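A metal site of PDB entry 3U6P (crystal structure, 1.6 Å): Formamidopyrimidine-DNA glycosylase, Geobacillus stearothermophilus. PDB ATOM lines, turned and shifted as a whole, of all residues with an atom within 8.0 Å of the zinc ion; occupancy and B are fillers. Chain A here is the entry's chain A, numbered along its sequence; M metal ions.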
ATOM      1  N   PHE A 181      10.576 -33.371  11.218  1.00  0.00           N
ATOM      2  CA  PHE A 181       9.418 -32.813  10.543  1.00  0.00           C
ATOM      3  C   PHE A 181       9.579 -32.865   9.028  1.00  0.00           C
ATOM      4  O   PHE A 181       8.688 -33.302   8.307  1.00  0.00           O
ATOM      5  CB  PHE A 181       9.150 -31.370  10.975  1.00  0.00           C
ATOM      6  CG  PHE A 181       8.121 -30.690  10.120  1.00  0.00           C
ATOM      7  CD1 PHE A 181       6.772 -30.840  10.385  1.00  0.00           C
ATOM      8  CD2 PHE A 181       8.512 -29.940   9.026  1.00  0.00           C
ATOM      9  CE1 PHE A 181       5.819 -30.221   9.594  1.00  0.00           C
ATOM     10  CE2 PHE A 181       7.565 -29.324   8.223  1.00  0.00           C
ATOM     11  CZ  PHE A 181       6.214 -29.459   8.507  1.00  0.00           C
ATOM     12  N   TYR A 239       9.913 -24.828  11.164  1.00  0.00           N
ATOM     13  CA  TYR A 239       8.634 -25.471  10.903  1.00  0.00           C
ATOM     14  C   TYR A 239       7.914 -25.860  12.198  1.00  0.00           C
ATOM     15  O   TYR A 239       6.693 -25.741  12.286  1.00  0.00           O
ATOM     16  CB  TYR A 239       8.817 -26.722  10.046  1.00  0.00           C
ATOM     17  CG  TYR A 239       9.206 -26.438   8.617  1.00  0.00           C
ATOM     18  CD1 TYR A 239       8.271 -25.965   7.704  1.00  0.00           C
ATOM     19  CD2 TYR A 239      10.506 -26.649   8.175  1.00  0.00           C
ATOM     20  CE1 TYR A 239       8.623 -25.701   6.399  1.00  0.00           C
ATOM     21  CE2 TYR A 239      10.867 -26.395   6.868  1.00  0.00           C
ATOM     22  CZ  TYR A 239       9.921 -25.925   5.983  1.00  0.00           C
ATOM     23  OH  TYR A 239      10.283 -25.671   4.677  1.00  0.00           O
ATOM     24  N   VAL A 240       8.665 -26.331  13.189  1.00  0.00           N
ATOM     25  CA  VAL A 240       8.041 -26.864  14.396  1.00  0.00           C
ATOM     26  C   VAL A 240       8.654 -26.374  15.703  1.00  0.00           C
ATOM     27  O   VAL A 240       7.940 -26.163  16.684  1.00  0.00           O
ATOM     28  CB  VAL A 240       8.005 -28.409  14.403  1.00  0.00           C
ATOM     29  CG1 VAL A 240       7.150 -28.921  13.250  1.00  0.00           C
ATOM     30  CG2 VAL A 240       9.413 -28.990  14.338  1.00  0.00           C
ATOM     31  N   PRO A 247      -0.150 -22.809  13.790  1.00  0.00           N
ATOM     32  CA  PRO A 247      -0.451 -23.686  12.644  1.00  0.00           C
ATOM     33  C   PRO A 247       0.808 -24.171  11.929  1.00  0.00           C
ATOM     34  O   PRO A 247       1.761 -23.416  11.743  1.00  0.00           O
ATOM     35  CB  PRO A 247      -1.279 -22.786  11.718  1.00  0.00           C
ATOM     36  CG  PRO A 247      -0.902 -21.398  12.097  1.00  0.00           C
ATOM     37  CD  PRO A 247      -0.620 -21.429  13.572  1.00  0.00           C
ATOM     38  N   CYS A 248       0.796 -25.432  11.527  1.00  0.00           N
ATOM     39  CA  CYS A 248       1.855 -25.978  10.700  1.00  0.00           C
ATOM     40  C   CYS A 248       1.941 -25.184   9.408  1.00  0.00           C
ATOM     41  O   CYS A 248       0.922 -24.826   8.812  1.00  0.00           O
ATOM     42  CB  CYS A 248       1.591 -27.452  10.401  1.00  0.00           C
ATOM     43  SG  CYS A 248       2.741 -28.188   9.242  1.00  0.00           S
ATOM     44  N   LYS A 249       3.166 -24.888   8.972  1.00  0.00           N
ATOM     45  CA  LYS A 249       3.380 -24.082   7.780  1.00  0.00           C
ATOM     46  C   LYS A 249       3.076 -24.859   6.505  1.00  0.00           C
ATOM     47  O   LYS A 249       2.966 -24.276   5.425  1.00  0.00           O
ATOM     48  CB  LYS A 249       4.815 -23.552   7.749  1.00  0.00           C
ATOM     49  CG  LYS A 249       5.119 -22.560   8.859  1.00  0.00           C
ATOM     50  CD  LYS A 249       6.529 -21.998   8.762  1.00  0.00           C
ATOM     51  CE  LYS A 249       6.778 -20.989   9.868  1.00  0.00           C
ATOM     52  NZ  LYS A 249       8.150 -20.405   9.780  1.00  0.00           N
ATOM     53  N   ARG A 250       2.937 -26.182   6.626  1.00  0.00           N
ATOM     54  CA  ARG A 250       2.640 -27.036   5.484  1.00  0.00           C
ATOM     55  C   ARG A 250       1.179 -27.482   5.411  1.00  0.00           C
ATOM     56  O   ARG A 250       0.642 -27.638   4.323  1.00  0.00           O
ATOM     57  CB  ARG A 250       3.558 -28.268   5.479  1.00  0.00           C
ATOM     58  CG  ARG A 250       5.041 -27.953   5.334  1.00  0.00           C
ATOM     59  CD  ARG A 250       5.508 -28.144   3.899  1.00  0.00           C
ATOM     60  NE  ARG A 250       6.931 -27.857   3.742  1.00  0.00           N
ATOM     61  CZ  ARG A 250       7.906 -28.758   3.910  1.00  0.00           C
ATOM     62  NH1 ARG A 250       7.600 -30.000   4.245  1.00  0.00           N
ATOM     63  NH2 ARG A 250       9.168 -28.408   3.746  1.00  0.00           N
ATOM     64  N   CYS A 251       0.531 -27.687   6.565  1.00  0.00           N
ATOM     65  CA  CYS A 251      -0.837 -28.227   6.548  1.00  0.00           C
ATOM     66  C   CYS A 251      -1.827 -27.485   7.435  1.00  0.00           C
ATOM     67  O   CYS A 251      -3.031 -27.766   7.386  1.00  0.00           O
ATOM     68  CB  CYS A 251      -0.825 -29.709   6.933  1.00  0.00           C
ATOM     69  SG  CYS A 251      -0.593 -30.006   8.698  1.00  0.00           S
ATOM     70  N   GLY A 252      -1.353 -26.554   8.255  1.00  0.00           N
ATOM     71  CA  GLY A 252      -2.227 -25.756   9.099  1.00  0.00           C
ATOM     72  C   GLY A 252      -2.637 -26.381  10.422  1.00  0.00           C
ATOM     73  O   GLY A 252      -3.280 -25.723  11.243  1.00  0.00           O
ATOM     74  N   THR A 253      -2.282 -27.645  10.632  1.00  0.00           N
ATOM     75  CA  THR A 253      -2.579 -28.339  11.871  1.00  0.00           C
ATOM     76  C   THR A 253      -1.751 -27.732  12.997  1.00  0.00           C
ATOM     77  O   THR A 253      -0.578 -27.435  12.808  1.00  0.00           O
ATOM     78  CB  THR A 253      -2.247 -29.835  11.765  1.00  0.00           C
ATOM     79  OG1 THR A 253      -3.026 -30.422  10.703  1.00  0.00           O
ATOM     80  CG2 THR A 253      -2.551 -30.553  13.071  1.00  0.00           C
ATOM     81  N   PRO A 254      -2.365 -27.516  14.171  1.00  0.00           N
ATOM     82  CA  PRO A 254      -1.584 -26.940  15.269  1.00  0.00           C
ATOM     83  C   PRO A 254      -0.372 -27.805  15.640  1.00  0.00           C
ATOM     84  O   PRO A 254      -0.500 -29.017  15.825  1.00  0.00           O
ATOM     85  CB  PRO A 254      -2.579 -26.911  16.434  1.00  0.00           C
ATOM     86  CG  PRO A 254      -3.913 -26.836  15.773  1.00  0.00           C
ATOM     87  CD  PRO A 254      -3.778 -27.668  14.520  1.00  0.00           C
ATOM     88  N   ILE A 255       0.796 -27.171  15.737  1.00  0.00           N
ATOM     89  CA  ILE A 255       1.997 -27.866  16.164  1.00  0.00           C
ATOM     90  C   ILE A 255       1.841 -28.255  17.626  1.00  0.00           C
ATOM     91  O   ILE A 255       1.295 -27.492  18.431  1.00  0.00           O
ATOM     92  CB  ILE A 255       3.244 -26.987  15.964  1.00  0.00           C
ATOM     93  CG1 ILE A 255       3.409 -26.646  14.479  1.00  0.00           C
ATOM     94  CG2 ILE A 255       4.496 -27.674  16.491  1.00  0.00           C
ATOM     95  CD1 ILE A 255       3.368 -27.861  13.570  1.00  0.00           C
ATOM     96  N   TYR A 267       6.327 -31.186  17.051  1.00  0.00           N
ATOM     97  CA  TYR A 267       5.995 -31.961  15.866  1.00  0.00           C
ATOM     98  C   TYR A 267       4.621 -31.595  15.327  1.00  0.00           C
ATOM     99  O   TYR A 267       3.780 -31.055  16.053  1.00  0.00           O
ATOM    100  CB  TYR A 267       6.048 -33.457  16.192  1.00  0.00           C
ATOM    101  CG  TYR A 267       5.030 -33.857  17.235  1.00  0.00           C
ATOM    102  CD1 TYR A 267       3.789 -34.353  16.859  1.00  0.00           C
ATOM    103  CD2 TYR A 267       5.314 -33.744  18.588  1.00  0.00           C
ATOM    104  CE1 TYR A 267       2.855 -34.712  17.808  1.00  0.00           C
ATOM    105  CE2 TYR A 267       4.375 -34.100  19.550  1.00  0.00           C
ATOM    106  CZ  TYR A 267       3.145 -34.593  19.146  1.00  0.00           C
ATOM    107  OH  TYR A 267       2.207 -34.954  20.087  1.00  0.00           O
ATOM    108  N   CYS A 268       4.392 -31.879  14.057  1.00  0.00           N
ATOM    109  CA  CYS A 268       3.052 -31.791  13.484  1.00  0.00           C
ATOM    110  C   CYS A 268       2.468 -33.182  13.396  1.00  0.00           C
ATOM    111  O   CYS A 268       3.039 -34.056  12.748  1.00  0.00           O
ATOM    112  CB  CYS A 268       3.098 -31.171  12.091  1.00  0.00           C
ATOM    113  SG  CYS A 268       1.498 -31.246  11.271  1.00  0.00           S
ATOM    114  N   PRO A 269       1.315 -33.404  14.050  1.00  0.00           N
ATOM    115  CA  PRO A 269       0.731 -34.743  14.116  1.00  0.00           C
ATOM    116  C   PRO A 269       0.113 -35.188  12.787  1.00  0.00           C
ATOM    117  O   PRO A 269      -0.264 -36.358  12.671  1.00  0.00           O
ATOM    118  CB  PRO A 269      -0.361 -34.600  15.187  1.00  0.00           C
ATOM    119  CG  PRO A 269      -0.729 -33.163  15.158  1.00  0.00           C
ATOM    120  CD  PRO A 269       0.544 -32.421  14.829  1.00  0.00           C
ATOM    121  N   ARG A 270       0.014 -34.292  11.824  1.00  0.00           N
ATOM    122  CA  ARG A 270      -0.480 -34.657  10.498  1.00  0.00           C
ATOM    123  C   ARG A 270       0.662 -34.969   9.522  1.00  0.00           C
ATOM    124  O   ARG A 270       0.639 -35.996   8.843  1.00  0.00           O
ATOM    125  CB  ARG A 270      -1.378 -33.566   9.905  1.00  0.00           C
ATOM    126  CG  ARG A 270      -1.932 -33.925   8.535  1.00  0.00           C
ATOM    127  CD  ARG A 270      -2.924 -32.912   8.016  1.00  0.00           C
ATOM    128  NE  ARG A 270      -3.461 -33.341   6.727  1.00  0.00           N
ATOM    129  CZ  ARG A 270      -4.405 -32.698   6.061  1.00  0.00           C
ATOM    130  NH1 ARG A 270      -4.830 -33.181   4.897  1.00  0.00           N
ATOM    131  NH2 ARG A 270      -4.932 -31.587   6.542  1.00  0.00           N
ATOM    132  N   CYS A 271       1.649 -34.078   9.451  1.00  0.00           N
ATOM    133  CA  CYS A 271       2.751 -34.227   8.512  1.00  0.00           C
ATOM    134  C   CYS A 271       3.692 -35.372   8.899  1.00  0.00           C
ATOM    135  O   CYS A 271       4.313 -35.989   8.042  1.00  0.00           O
ATOM    136  CB  CYS A 271       3.559 -32.926   8.419  1.00  0.00           C
ATOM    137  SG  CYS A 271       2.747 -31.599   7.496  1.00  0.00           S
ATOM    138  N   GLN A 272       3.803 -35.625  10.197  1.00  0.00           N
ATOM    139  CA  GLN A 272       4.717 -36.660  10.688  1.00  0.00           C
ATOM    140  C   GLN A 272       3.956 -37.906  11.128  1.00  0.00           C
ATOM    141  O   GLN A 272       2.912 -37.816  11.767  1.00  0.00           O
ATOM    142  CB  GLN A 272       5.570 -36.110  11.831  1.00  0.00           C
ATOM    143  CG  GLN A 272       6.487 -34.979  11.393  1.00  0.00           C
ATOM    144  CD  GLN A 272       7.081 -34.208  12.558  1.00  0.00           C
ATOM    145  OE1 GLN A 272       6.664 -33.099  12.858  1.00  0.00           O
ATOM    146  NE2 GLN A 272       8.085 -34.791  13.204  1.00  0.00           N
HETATM  147 ZN    ZN M   1       1.700 -30.329   9.151  1.00  0.00          ZN
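Of the 18 residues printed, 4 come within 4 Å of the zinc ion.
The zinc ion is bound by SG of Cys 268 (2.3 Å), SG of Cys 271 (2.3 Å), SG of Cys 251 (2.4 Å) and SG of Cys 248 (2.4 Å). The zinc ion has four donor atoms within binding distance.
The backbone NH (N) of Arg 270 sits close to the side-chain sulfur (SG) of Cys 268, 3.4 Å away. N of Cys 268 sits at hydrogen-bond distance from OE1 of Gln 272 (2.8 Å). The side-chain hydroxyl (OG1) of Thr 253 sits close to the side-chain sulfur (SG) of Cys 251 (3.2 Å). SG of Cys 248 sits close to N of Arg 250, 3.3 Å away. N of Cys 248 is in hydrogen-bond range of O of Thr 253 (2.7 Å).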
